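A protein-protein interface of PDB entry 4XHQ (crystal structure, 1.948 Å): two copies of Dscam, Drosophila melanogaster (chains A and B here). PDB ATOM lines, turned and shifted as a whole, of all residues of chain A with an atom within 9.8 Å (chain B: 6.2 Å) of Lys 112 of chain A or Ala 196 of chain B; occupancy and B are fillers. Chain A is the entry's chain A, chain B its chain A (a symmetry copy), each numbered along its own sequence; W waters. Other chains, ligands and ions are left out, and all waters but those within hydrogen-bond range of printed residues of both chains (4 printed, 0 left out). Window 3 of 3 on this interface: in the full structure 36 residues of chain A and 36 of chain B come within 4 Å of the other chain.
A ring nitrogen (NE2) of His 114 of chain A is in hydrogen-bond range of the side-chain carboxylate of Asp 109 of chain B (2.7 Å). The side-chain amino group (NZ) of Lys 112 of chain A is in salt-bridge range of the side-chain carboxylate (OE2) of Glu 107 of chain B. The side-chain carboxylate of Asp 109 of chain B is in salt-bridge range of the side-chain amino group of Lys 112 of chain A. The side-chain amide oxygen (OD1) of Asn 111 of chain B sits close to the side-chain amide oxygen (OD1) of Asn 111 of chain A (2.7 Å).
The side-chain hydroxyl (OH) of Tyr 105 of chain B lies within hydrogen-bond range of the side-chain carboxylate (OE1) of Glu 107 of chain B (2.6 Å). The side-chain hydroxyl (OG1) of Thr 197 of chain B lies within hydrogen-bond range of the backbone NH (N) of Val 110 of chain B, at 3.0 Å. O of Ala 108 of chain B lies within hydrogen-bond range of N of Ala 196 of chain B (2.8 Å). The side-chain hydroxyl of Ser 195 of chain B sits at hydrogen-bond distance from the backbone carbonyl oxygen of Thr 197 of chain B (3.0 Å). OD1 of Asp 109 of chain B sits at hydrogen-bond distance from OG1 of Thr 197 of chain B.
Among the printed residues, pairs that only touch across the chains: His 114 of chain A with Glu 107 of chain B (3.6 Å), Lys 112 of chain A with Ala 196 of chain B (3.7 Å) and Lys 112 of chain A with Thr 197 of chain B (3.8 Å).
Lys 112 of chain A touches four residues of chain B. Ala 196 of chain B touches just one residue of chain A: Lys 112. No residue of chain A comes within 4 Å of Ser 195 of chain B. Thr 197 of chain B touches just one residue of chain A: Lys 112 (3.8 Å). Of the printed residues of chain B, Asn 111 of chain A touches Asn 111. Printed residues of chain A within 4 Å of Asp 109 of chain B: Lys 112 (2.7 Å) and His 114 (2.7 Å). Gly 176 of chain A touches none of the printed residues of chain B. Trp 140 of chain A touches none of the printed residues of chain B. The nearest residue of chain A that does not touch Ala 196 of chain B is His 114 of chain A (6.5 Å).
Hydrophobic or aromatic side chains of chain A within 4 Å of the printed part of chain B: His 114. Hydrophobic or aromatic side chains of chain B that line the printed part of chain A: Ala 196. Among the printed residues, 7 pairs touch across the chains.
Asn 111 of chain B touches its own counterpart, Asn 111 of chain A.
Water W3 lies within hydrogen-bond range of O of Lys 112 of chain A (2.8 Å) and OD1 of Asn 111 of chain B (3.2 Å). Water W1 lies within hydrogen-bond range of N of Lys 112 of chain A (2.8 Å) and ND2 of Asn 111 of chain B (3.1 Å). Water W4 lies within hydrogen-bond range of ND1 of His 114 of chain A (3.2 Å) and N of Glu 107 of chain B (3.2 Å). Water W2 lies within hydrogen-bond range of NE2 of His 114 of chain A (3.2 Å) and OD2 of Asp 109 of chain B (3.3 Å).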
ATOM      1  N   ASP A 109      15.561 -17.353   4.096  1.00  0.00           N
ATOM      2  CA  ASP A 109      14.286 -17.927   4.559  1.00  0.00           C
ATOM      3  C   ASP A 109      13.204 -16.845   4.607  1.00  0.00           C
ATOM      4  O   ASP A 109      13.502 -15.650   4.716  1.00  0.00           O
ATOM      5  CB  ASP A 109      14.465 -18.551   5.964  1.00  0.00           C
ATOM      6  CG  ASP A 109      15.196 -19.895   5.907  1.00  0.00           C
ATOM      7  OD1 ASP A 109      14.823 -20.748   5.048  1.00  0.00           O
ATOM      8  OD2 ASP A 109      16.148 -20.085   6.691  1.00  0.00           O
ATOM      9  N   VAL A 110      11.942 -17.250   4.500  1.00  0.00           N
ATOM     10  CA  VAL A 110      10.799 -16.331   4.731  1.00  0.00           C
ATOM     11  C   VAL A 110       9.934 -17.083   5.738  1.00  0.00           C
ATOM     12  O   VAL A 110       9.521 -18.206   5.449  1.00  0.00           O
ATOM     13  CB  VAL A 110       9.993 -16.010   3.455  1.00  0.00           C
ATOM     14  CG1 VAL A 110       8.862 -14.975   3.768  1.00  0.00           C
ATOM     15  CG2 VAL A 110      10.910 -15.471   2.308  1.00  0.00           C
ATOM     16  N   ASN A 111       9.746 -16.506   6.923  1.00  0.00           N
ATOM     17  CA  ASN A 111       8.993 -17.140   7.958  1.00  0.00           C
ATOM     18  C   ASN A 111       7.545 -16.605   8.026  1.00  0.00           C
ATOM     19  O   ASN A 111       7.179 -15.646   7.336  1.00  0.00           O
ATOM     20  CB  ASN A 111       9.686 -16.932   9.294  1.00  0.00           C
ATOM     21  CG  ASN A 111      11.083 -17.564   9.326  1.00  0.00           C
ATOM     22  OD1 ASN A 111      11.961 -17.074  10.018  1.00  0.00           O
ATOM     23  ND2 ASN A 111      11.284 -18.638   8.558  1.00  0.00           N
ATOM     24  N   LYS A 112       6.764 -17.227   8.881  1.00  0.00           N
ATOM     25  CA  LYS A 112       5.372 -16.809   9.115  1.00  0.00           C
ATOM     26  C   LYS A 112       5.388 -15.410   9.755  1.00  0.00           C
ATOM     27  O   LYS A 112       6.173 -15.155  10.681  1.00  0.00           O
ATOM     28  CB  LYS A 112       4.655 -17.792  10.060  1.00  0.00           C
ATOM     29  CG  LYS A 112       4.408 -19.191   9.494  1.00  0.00           C
ATOM     30  CD  LYS A 112       4.328 -20.276  10.595  1.00  0.00           C
ATOM     31  CE  LYS A 112       3.178 -20.010  11.565  1.00  0.00           C
ATOM     32  NZ  LYS A 112       2.952 -21.145  12.572  1.00  0.00           N
ATOM     33  N   GLU A 113       4.468 -14.561   9.326  1.00  0.00           N
ATOM     34  CA  GLU A 113       4.330 -13.210   9.857  1.00  0.00           C
ATOM     35  C   GLU A 113       2.953 -13.063  10.566  1.00  0.00           C
ATOM     36  O   GLU A 113       1.921 -13.186   9.908  1.00  0.00           O
ATOM     37  CB  GLU A 113       4.452 -12.222   8.717  1.00  0.00           C
ATOM     38  CG  GLU A 113       4.503 -10.775   9.138  1.00  0.00           C
ATOM     39  CD  GLU A 113       5.746 -10.478   9.994  1.00  0.00           C
ATOM     40  OE1 GLU A 113       6.774 -11.208   9.842  1.00  0.00           O
ATOM     41  OE2 GLU A 113       5.678  -9.529  10.821  1.00  0.00           O
ATOM     42  N   HIS A 114       2.934 -12.829  11.878  1.00  0.00           N
ATOM     43  CA  HIS A 114       1.644 -12.778  12.608  1.00  0.00           C
ATOM     44  C   HIS A 114       1.180 -11.347  12.696  1.00  0.00           C
ATOM     45  O   HIS A 114       1.937 -10.492  13.153  1.00  0.00           O
ATOM     46  CB  HIS A 114       1.764 -13.334  13.996  1.00  0.00           C
ATOM     47  CG  HIS A 114       2.075 -14.784  14.029  1.00  0.00           C
ATOM     48  ND1 HIS A 114       1.112 -15.743  14.283  1.00  0.00           N
ATOM     49  CD2 HIS A 114       3.242 -15.443  13.834  1.00  0.00           C
ATOM     50  CE1 HIS A 114       1.682 -16.937  14.260  1.00  0.00           C
ATOM     51  NE2 HIS A 114       2.968 -16.782  13.981  1.00  0.00           N
ATOM     52  N   VAL A 115      -0.034 -11.091  12.224  1.00  0.00           N
ATOM     53  CA  VAL A 115      -0.533  -9.718  12.105  1.00  0.00           C
ATOM     54  C   VAL A 115      -1.987  -9.689  12.556  1.00  0.00           C
ATOM     55  O   VAL A 115      -2.688 -10.729  12.532  1.00  0.00           O
ATOM     56  CB  VAL A 115      -0.415  -9.176  10.665  1.00  0.00           C
ATOM     57  CG1 VAL A 115       1.069  -9.102  10.191  1.00  0.00           C
ATOM     58  CG2 VAL A 115      -1.206 -10.028   9.685  1.00  0.00           C
ATOM     59  N   ALA A 121       1.474  -5.129   7.029  1.00  0.00           N
ATOM     60  CA  ALA A 121       2.365  -6.265   7.305  1.00  0.00           C
ATOM     61  C   ALA A 121       3.656  -6.023   6.548  1.00  0.00           C
ATOM     62  O   ALA A 121       3.651  -5.417   5.487  1.00  0.00           O
ATOM     63  CB  ALA A 121       1.753  -7.612   6.863  1.00  0.00           C
ATOM     64  N   VAL A 122       4.745  -6.555   7.099  1.00  0.00           N
ATOM     65  CA  VAL A 122       6.019  -6.506   6.424  1.00  0.00           C
ATOM     66  C   VAL A 122       6.568  -7.942   6.371  1.00  0.00           C
ATOM     67  O   VAL A 122       6.743  -8.586   7.408  1.00  0.00           O
ATOM     68  CB  VAL A 122       6.985  -5.570   7.169  1.00  0.00           C
ATOM     69  CG1 VAL A 122       8.376  -5.642   6.554  1.00  0.00           C
ATOM     70  CG2 VAL A 122       6.399  -4.135   7.147  1.00  0.00           C
ATOM     71  N   ILE A 123       6.740  -8.440   5.149  1.00  0.00           N
ATOM     72  CA  ILE A 123       7.289  -9.779   4.930  1.00  0.00           C
ATOM     73  C   ILE A 123       8.797  -9.586   4.713  1.00  0.00           C
ATOM     74  O   ILE A 123       9.181  -8.828   3.842  1.00  0.00           O
ATOM     75  CB  ILE A 123       6.712 -10.485   3.676  1.00  0.00           C
ATOM     76  CG1 ILE A 123       5.186 -10.356   3.617  1.00  0.00           C
ATOM     77  CG2 ILE A 123       7.090 -11.975   3.707  1.00  0.00           C
ATOM     78  CD1 ILE A 123       4.598 -11.094   4.687  1.00  0.00           C
ATOM     79  N   LYS A 124       9.608 -10.329   5.456  1.00  0.00           N
ATOM     80  CA  LYS A 124      11.044 -10.151   5.398  1.00  0.00           C
ATOM     81  C   LYS A 124      11.746 -11.348   4.798  1.00  0.00           C
ATOM     82  O   LYS A 124      11.490 -12.514   5.144  1.00  0.00           O
ATOM     83  CB  LYS A 124      11.605  -9.909   6.804  1.00  0.00           C
ATOM     84  CG  LYS A 124      11.185  -8.531   7.386  1.00  0.00           C
ATOM     85  CD  LYS A 124      11.401  -8.410   8.920  1.00  0.00           C
ATOM     86  CE  LYS A 124      10.245  -9.006   9.746  1.00  0.00           C
ATOM     87  NZ  LYS A 124       8.923  -8.286   9.607  1.00  0.00           N
ATOM     88  N   LEU A 126      14.955 -13.302   5.172  1.00  0.00           N
ATOM     89  CA  LEU A 126      16.003 -13.470   6.183  1.00  0.00           C
ATOM     90  C   LEU A 126      17.291 -14.050   5.566  1.00  0.00           C
ATOM     91  O   LEU A 126      17.316 -15.213   5.149  1.00  0.00           O
ATOM     92  CB  LEU A 126      15.532 -14.397   7.272  1.00  0.00           C
ATOM     93  CG  LEU A 126      14.225 -13.873   7.920  1.00  0.00           C
ATOM     94  CD1 LEU A 126      13.751 -14.838   8.976  1.00  0.00           C
ATOM     95  CD2 LEU A 126      14.319 -12.453   8.512  1.00  0.00           C
ATOM     96  N   TRP A 140       9.958 -10.399  -5.237  1.00  0.00           N
ATOM     97  CA  TRP A 140       9.126 -11.177  -4.331  1.00  0.00           C
ATOM     98  C   TRP A 140       8.097 -11.923  -5.226  1.00  0.00           C
ATOM     99  O   TRP A 140       7.715 -11.393  -6.248  1.00  0.00           O
ATOM    100  CB  TRP A 140       8.372 -10.272  -3.359  1.00  0.00           C
ATOM    101  CG  TRP A 140       9.200  -9.955  -2.145  1.00  0.00           C
ATOM    102  CD1 TRP A 140       9.976  -8.828  -1.977  1.00  0.00           C
ATOM    103  CD2 TRP A 140       9.370 -10.746  -0.990  1.00  0.00           C
ATOM    104  NE1 TRP A 140      10.624  -8.881  -0.771  1.00  0.00           N
ATOM    105  CE2 TRP A 140      10.267 -10.035  -0.124  1.00  0.00           C
ATOM    106  CE3 TRP A 140       8.840 -11.975  -0.560  1.00  0.00           C
ATOM    107  CZ2 TRP A 140      10.633 -10.502   1.133  1.00  0.00           C
ATOM    108  CZ3 TRP A 140       9.226 -12.479   0.684  1.00  0.00           C
ATOM    109  CH2 TRP A 140      10.127 -11.732   1.537  1.00  0.00           C
ATOM    110  N   GLY A 176      -4.256 -14.474   4.077  1.00  0.00           N
ATOM    111  CA  GLY A 176      -3.647 -15.628   4.731  1.00  0.00           C
ATOM    112  C   GLY A 176      -3.552 -16.864   3.822  1.00  0.00           C
ATOM    113  O   GLY A 176      -2.943 -17.852   4.213  1.00  0.00           O
ATOM    114  N   LYS A 178      -2.097 -17.036   0.832  1.00  0.00           N
ATOM    115  CA  LYS A 178      -0.986 -16.869  -0.125  1.00  0.00           C
ATOM    116  C   LYS A 178       0.289 -17.202   0.617  1.00  0.00           C
ATOM    117  O   LYS A 178       0.335 -17.067   1.845  1.00  0.00           O
ATOM    118  CB  LYS A 178      -0.911 -15.436  -0.670  1.00  0.00           C
ATOM    119  CG  LYS A 178      -2.062 -15.022  -1.545  1.00  0.00           C
ATOM    120  CD  LYS A 178      -1.914 -13.570  -1.924  1.00  0.00           C
ATOM    121  CE  LYS A 178      -2.941 -13.134  -2.957  1.00  0.00           C
ATOM    122  NZ  LYS A 178      -4.329 -13.122  -2.400  1.00  0.00           N
ATOM    123  N   SER A 179       1.296 -17.716  -0.080  1.00  0.00           N
ATOM    124  CA  SER A 179       2.591 -17.773   0.575  1.00  0.00           C
ATOM    125  C   SER A 179       3.587 -17.027  -0.304  1.00  0.00           C
ATOM    126  O   SER A 179       3.354 -16.843  -1.505  1.00  0.00           O
ATOM    127  CB  SER A 179       3.015 -19.233   0.906  1.00  0.00           C
ATOM    128  OG  SER A 179       3.585 -19.887  -0.189  1.00  0.00           O
ATOM    129  N   TYR A 180       4.679 -16.559   0.310  1.00  0.00           N
ATOM    130  CA  TYR A 180       5.571 -15.567  -0.329  1.00  0.00           C
ATOM    131  C   TYR A 180       6.987 -16.085  -0.388  1.00  0.00           C
ATOM    132  O   TYR A 180       7.453 -16.601   0.591  1.00  0.00           O
ATOM    133  CB  TYR A 180       5.547 -14.227   0.463  1.00  0.00           C
ATOM    134  CG  TYR A 180       4.211 -13.512   0.399  1.00  0.00           C
ATOM    135  CD1 TYR A 180       3.233 -13.766   1.327  1.00  0.00           C
ATOM    136  CD2 TYR A 180       3.931 -12.617  -0.618  1.00  0.00           C
ATOM    137  CE1 TYR A 180       2.004 -13.157   1.240  1.00  0.00           C
ATOM    138  CE2 TYR A 180       2.701 -11.995  -0.715  1.00  0.00           C
ATOM    139  CZ  TYR A 180       1.741 -12.282   0.208  1.00  0.00           C
ATOM    140  OH  TYR A 180       0.494 -11.653   0.149  1.00  0.00           O
ATOM    141  N   THR A 197      12.520 -21.368   2.182  1.00  0.00           N
ATOM    142  CA  THR A 197      11.185 -21.555   2.775  1.00  0.00           C
ATOM    143  C   THR A 197      10.274 -20.475   2.228  1.00  0.00           C
ATOM    144  O   THR A 197      10.759 -19.413   1.794  1.00  0.00           O
ATOM    145  CB  THR A 197      11.254 -21.438   4.320  1.00  0.00           C
ATOM    146  OG1 THR A 197      11.959 -20.209   4.645  1.00  0.00           O
ATOM    147  CG2 THR A 197      12.038 -22.645   4.943  1.00  0.00           C
ATOM    148  N   LYS A 198       8.959 -20.683   2.342  1.00  0.00           N
ATOM    149  CA  LYS A 198       7.988 -19.665   1.970  1.00  0.00           C
ATOM    150  C   LYS A 198       7.280 -19.145   3.228  1.00  0.00           C
ATOM    151  O   LYS A 198       7.050 -19.903   4.144  1.00  0.00           O
ATOM    152  CB  LYS A 198       6.938 -20.249   0.998  1.00  0.00           C
ATOM    153  CG  LYS A 198       7.480 -20.647  -0.343  1.00  0.00           C
ATOM    154  CD  LYS A 198       6.754 -21.845  -0.865  1.00  0.00           C
ATOM    155  CE  LYS A 198       5.709 -21.496  -1.860  1.00  0.00           C
ATOM    156  NZ  LYS A 198       5.665 -22.477  -3.050  1.00  0.00           N
ATOM    157  N   GLY A 199       6.868 -17.889   3.231  1.00  0.00           N
ATOM    158  CA  GLY A 199       6.287 -17.312   4.429  1.00  0.00           C
ATOM    159  C   GLY A 199       4.815 -17.082   4.138  1.00  0.00           C
ATOM    160  O   GLY A 199       4.439 -16.877   2.998  1.00  0.00           O
ATOM    161  N   ARG A 200       3.983 -17.102   5.163  1.00  0.00           N
ATOM    162  CA  ARG A 200       2.600 -16.697   4.971  1.00  0.00           C
ATOM    163  C   ARG A 200       2.241 -15.729   6.064  1.00  0.00           C
ATOM    164  O   ARG A 200       2.914 -15.711   7.112  1.00  0.00           O
ATOM    165  CB  ARG A 200       1.671 -17.929   4.954  1.00  0.00           C
ATOM    166  CG  ARG A 200       1.719 -18.810   6.182  1.00  0.00           C
ATOM    167  CD  ARG A 200       0.941 -20.160   5.937  1.00  0.00           C
ATOM    168  NE  ARG A 200       1.174 -21.142   7.009  1.00  0.00           N
ATOM    169  CZ  ARG A 200       0.413 -21.249   8.098  1.00  0.00           C
ATOM    170  NH1 ARG A 200      -0.641 -20.446   8.248  1.00  0.00           N
ATOM    171  NH2 ARG A 200       0.693 -22.154   9.041  1.00  0.00           N
ATOM    172  N   LEU A 201       1.280 -14.842   5.787  1.00  0.00           N
ATOM    173  CA  LEU A 201       0.645 -14.061   6.862  1.00  0.00           C
ATOM    174  C   LEU A 201      -0.285 -14.945   7.663  1.00  0.00           C
ATOM    175  O   LEU A 201      -1.080 -15.665   7.060  1.00  0.00           O
ATOM    176  CB  LEU A 201      -0.164 -12.927   6.267  1.00  0.00           C
ATOM    177  CG  LEU A 201       0.668 -12.007   5.421  1.00  0.00           C
ATOM    178  CD1 LEU A 201      -0.239 -11.179   4.488  1.00  0.00           C
ATOM    179  CD2 LEU A 201       1.437 -11.124   6.416  1.00  0.00           C
ATOM    180  N   VAL A 202      -0.177 -14.921   8.992  1.00  0.00           N
ATOM    181  CA  VAL A 202      -1.106 -15.582   9.884  1.00  0.00           C
ATOM    182  C   VAL A 202      -1.943 -14.442  10.524  1.00  0.00           C
ATOM    183  O   VAL A 202      -1.442 -13.641  11.300  1.00  0.00           O
ATOM    184  CB  VAL A 202      -0.420 -16.411  10.963  1.00  0.00           C
ATOM    185  CG1 VAL A 202      -1.469 -17.085  11.869  1.00  0.00           C
ATOM    186  CG2 VAL A 202       0.573 -17.478  10.319  1.00  0.00           C
ATOM    187  N   ILE A 203      -3.227 -14.393  10.198  1.00  0.00           N
ATOM    188  CA  ILE A 203      -4.036 -13.242  10.595  1.00  0.00           C
ATOM    189  C   ILE A 203      -4.850 -13.496  11.824  1.00  0.00           C
ATOM    190  O   ILE A 203      -5.622 -14.475  11.905  1.00  0.00           O
ATOM    191  CB  ILE A 203      -4.883 -12.830   9.449  1.00  0.00           C
ATOM    192  CG1 ILE A 203      -3.925 -12.434   8.335  1.00  0.00           C
ATOM    193  CG2 ILE A 203      -5.819 -11.685   9.899  1.00  0.00           C
ATOM    194  CD1 ILE A 203      -4.440 -12.608   6.981  1.00  0.00           C
ATOM    195  N   TYR B 105      -6.955 -17.935  20.663  1.00  0.00           N
ATOM    196  CA  TYR B 105      -5.872 -18.789  20.205  1.00  0.00           C
ATOM    197  C   TYR B 105      -4.655 -17.954  19.774  1.00  0.00           C
ATOM    198  O   TYR B 105      -4.799 -16.938  19.080  1.00  0.00           O
ATOM    199  CB  TYR B 105      -6.379 -19.637  19.023  1.00  0.00           C
ATOM    200  CG  TYR B 105      -5.283 -20.474  18.388  1.00  0.00           C
ATOM    201  CD1 TYR B 105      -4.965 -21.723  18.925  1.00  0.00           C
ATOM    202  CD2 TYR B 105      -4.560 -20.006  17.278  1.00  0.00           C
ATOM    203  CE1 TYR B 105      -3.940 -22.548  18.343  1.00  0.00           C
ATOM    204  CE2 TYR B 105      -3.502 -20.821  16.677  1.00  0.00           C
ATOM    205  CZ  TYR B 105      -3.212 -22.072  17.245  1.00  0.00           C
ATOM    206  OH  TYR B 105      -2.228 -22.899  16.707  1.00  0.00           O
ATOM    207  N   GLU B 107      -0.278 -18.678  18.566  1.00  0.00           N
ATOM    208  CA  GLU B 107       0.798 -19.642  18.535  1.00  0.00           C
ATOM    209  C   GLU B 107       2.157 -18.953  18.501  1.00  0.00           C
ATOM    210  O   GLU B 107       2.330 -17.829  18.004  1.00  0.00           O
ATOM    211  CB  GLU B 107       0.599 -20.601  17.349  1.00  0.00           C
ATOM    212  CG  GLU B 107       0.599 -19.863  16.060  1.00  0.00           C
ATOM    213  CD  GLU B 107       0.126 -20.692  14.830  1.00  0.00           C
ATOM    214  OE1 GLU B 107      -0.657 -21.695  14.954  1.00  0.00           O
ATOM    215  OE2 GLU B 107       0.566 -20.306  13.714  1.00  0.00           O
ATOM    216  N   ALA B 108       3.102 -19.643  19.100  1.00  0.00           N
ATOM    217  CA  ALA B 108       4.512 -19.239  19.089  1.00  0.00           C
ATOM    218  C   ALA B 108       5.225 -20.057  17.983  1.00  0.00           C
ATOM    219  O   ALA B 108       4.758 -21.159  17.639  1.00  0.00           O
ATOM    220  CB  ALA B 108       5.123 -19.493  20.499  1.00  0.00           C
ATOM    221  N   ASP B 109       6.282 -19.505  17.378  1.00  0.00           N
ATOM    222  CA  ASP B 109       7.021 -20.229  16.330  1.00  0.00           C
ATOM    223  C   ASP B 109       8.498 -20.354  16.713  1.00  0.00           C
ATOM    224  O   ASP B 109       9.022 -19.558  17.500  1.00  0.00           O
ATOM    225  CB  ASP B 109       6.891 -19.485  14.979  1.00  0.00           C
ATOM    226  CG  ASP B 109       5.518 -19.698  14.336  1.00  0.00           C
ATOM    227  OD1 ASP B 109       5.054 -20.875  14.280  1.00  0.00           O
ATOM    228  OD2 ASP B 109       4.901 -18.698  13.916  1.00  0.00           O
ATOM    229  N   VAL B 110       9.175 -21.368  16.182  1.00  0.00           N
ATOM    230  CA  VAL B 110      10.649 -21.484  16.312  1.00  0.00           C
ATOM    231  C   VAL B 110      11.121 -21.686  14.875  1.00  0.00           C
ATOM    232  O   VAL B 110      10.678 -22.637  14.230  1.00  0.00           O
ATOM    233  CB  VAL B 110      11.103 -22.658  17.203  1.00  0.00           C
ATOM    234  CG1 VAL B 110      12.660 -22.661  17.356  1.00  0.00           C
ATOM    235  CG2 VAL B 110      10.427 -22.614  18.613  1.00  0.00           C
ATOM    236  N   ASN B 111      11.929 -20.759  14.367  1.00  0.00           N
ATOM    237  CA  ASN B 111      12.395 -20.822  13.018  1.00  0.00           C
ATOM    238  C   ASN B 111      13.823 -21.403  12.930  1.00  0.00           C
ATOM    239  O   ASN B 111      14.488 -21.638  13.946  1.00  0.00           O
ATOM    240  CB  ASN B 111      12.360 -19.434  12.401  1.00  0.00           C
ATOM    241  CG  ASN B 111      10.938 -18.862  12.342  1.00  0.00           C
ATOM    242  OD1 ASN B 111      10.759 -17.656  12.413  1.00  0.00           O
ATOM    243  ND2 ASN B 111       9.934 -19.735  12.233  1.00  0.00           N
ATOM    244  N   ARG B 193       1.151 -24.375  25.911  1.00  0.00           N
ATOM    245  CA  ARG B 193       1.120 -25.056  24.614  1.00  0.00           C
ATOM    246  C   ARG B 193       2.539 -25.114  24.091  1.00  0.00           C
ATOM    247  O   ARG B 193       3.425 -24.366  24.558  1.00  0.00           O
ATOM    248  CB  ARG B 193       0.233 -24.337  23.600  1.00  0.00           C
ATOM    249  CG  ARG B 193       0.542 -22.879  23.590  1.00  0.00           C
ATOM    250  CD  ARG B 193      -0.036 -22.168  22.405  1.00  0.00           C
ATOM    251  NE  ARG B 193       0.370 -22.773  21.149  1.00  0.00           N
ATOM    252  CZ  ARG B 193      -0.410 -23.449  20.294  1.00  0.00           C
ATOM    253  NH1 ARG B 193      -1.703 -23.728  20.577  1.00  0.00           N
ATOM    254  NH2 ARG B 193       0.188 -23.936  19.183  1.00  0.00           N
ATOM    255  N   LEU B 194       2.762 -26.026  23.157  1.00  0.00           N
ATOM    256  CA  LEU B 194       4.054 -26.122  22.458  1.00  0.00           C
ATOM    257  C   LEU B 194       4.009 -25.258  21.235  1.00  0.00           C
ATOM    258  O   LEU B 194       2.936 -24.985  20.671  1.00  0.00           O
ATOM    259  CB  LEU B 194       4.333 -27.605  22.062  1.00  0.00           C
ATOM    260  CG  LEU B 194       4.343 -28.463  23.332  1.00  0.00           C
ATOM    261  CD1 LEU B 194       4.258 -29.985  22.980  1.00  0.00           C
ATOM    262  CD2 LEU B 194       5.618 -28.173  24.049  1.00  0.00           C
ATOM    263  N   SER B 195       5.173 -24.913  20.717  1.00  0.00           N
ATOM    264  CA  SER B 195       5.192 -24.010  19.589  1.00  0.00           C
ATOM    265  C   SER B 195       4.652 -24.684  18.332  1.00  0.00           C
ATOM    266  O   SER B 195       4.735 -25.926  18.178  1.00  0.00           O
ATOM    267  CB  SER B 195       6.607 -23.481  19.337  1.00  0.00           C
ATOM    268  OG  SER B 195       7.512 -24.586  19.258  1.00  0.00           O
ATOM    269  N   ALA B 196       4.046 -23.869  17.469  1.00  0.00           N
ATOM    270  CA  ALA B 196       3.381 -24.382  16.258  1.00  0.00           C
ATOM    271  C   ALA B 196       4.427 -24.984  15.295  1.00  0.00           C
ATOM    272  O   ALA B 196       4.154 -25.936  14.619  1.00  0.00           O
ATOM    273  CB  ALA B 196       2.576 -23.257  15.555  1.00  0.00           C
ATOM    274  N   THR B 197       5.637 -24.421  15.270  1.00  0.00           N
ATOM    275  CA  THR B 197       6.690 -24.921  14.368  1.00  0.00           C
ATOM    276  C   THR B 197       7.876 -25.333  15.215  1.00  0.00           C
ATOM    277  O   THR B 197       8.032 -24.842  16.349  1.00  0.00           O
ATOM    278  CB  THR B 197       7.126 -23.812  13.375  1.00  0.00           C
ATOM    279  OG1 THR B 197       7.423 -22.614  14.143  1.00  0.00           O
ATOM    280  CG2 THR B 197       5.980 -23.484  12.357  1.00  0.00           C
ATOM    281  N   LYS B 198       8.770 -26.144  14.643  1.00  0.00           N
ATOM    282  CA  LYS B 198      10.012 -26.507  15.310  1.00  0.00           C
ATOM    283  C   LYS B 198      11.198 -25.870  14.574  1.00  0.00           C
ATOM    284  O   LYS B 198      11.162 -25.753  13.369  1.00  0.00           O
ATOM    285  CB  LYS B 198      10.187 -28.042  15.328  1.00  0.00           C
ATOM    286  CG  LYS B 198       9.178 -28.778  16.158  1.00  0.00           C
ATOM    287  CD  LYS B 198       8.863 -30.103  15.544  1.00  0.00           C
ATOM    288  CE  LYS B 198       9.589 -31.225  16.191  1.00  0.00           C
ATOM    289  NZ  LYS B 198       8.710 -32.480  16.374  1.00  0.00           N
HETATM  290  O   HOH W   1       7.772 -19.614  10.037  1.00  0.00           O
HETATM  291  O   HOH W   2       5.172 -16.399  16.263  1.00  0.00           O
HETATM  292  O   HOH W   3       7.580 -17.015  12.242  1.00  0.00           O
HETATM  293  O   HOH W   4      -0.791 -16.009  16.788  1.00  0.00           O
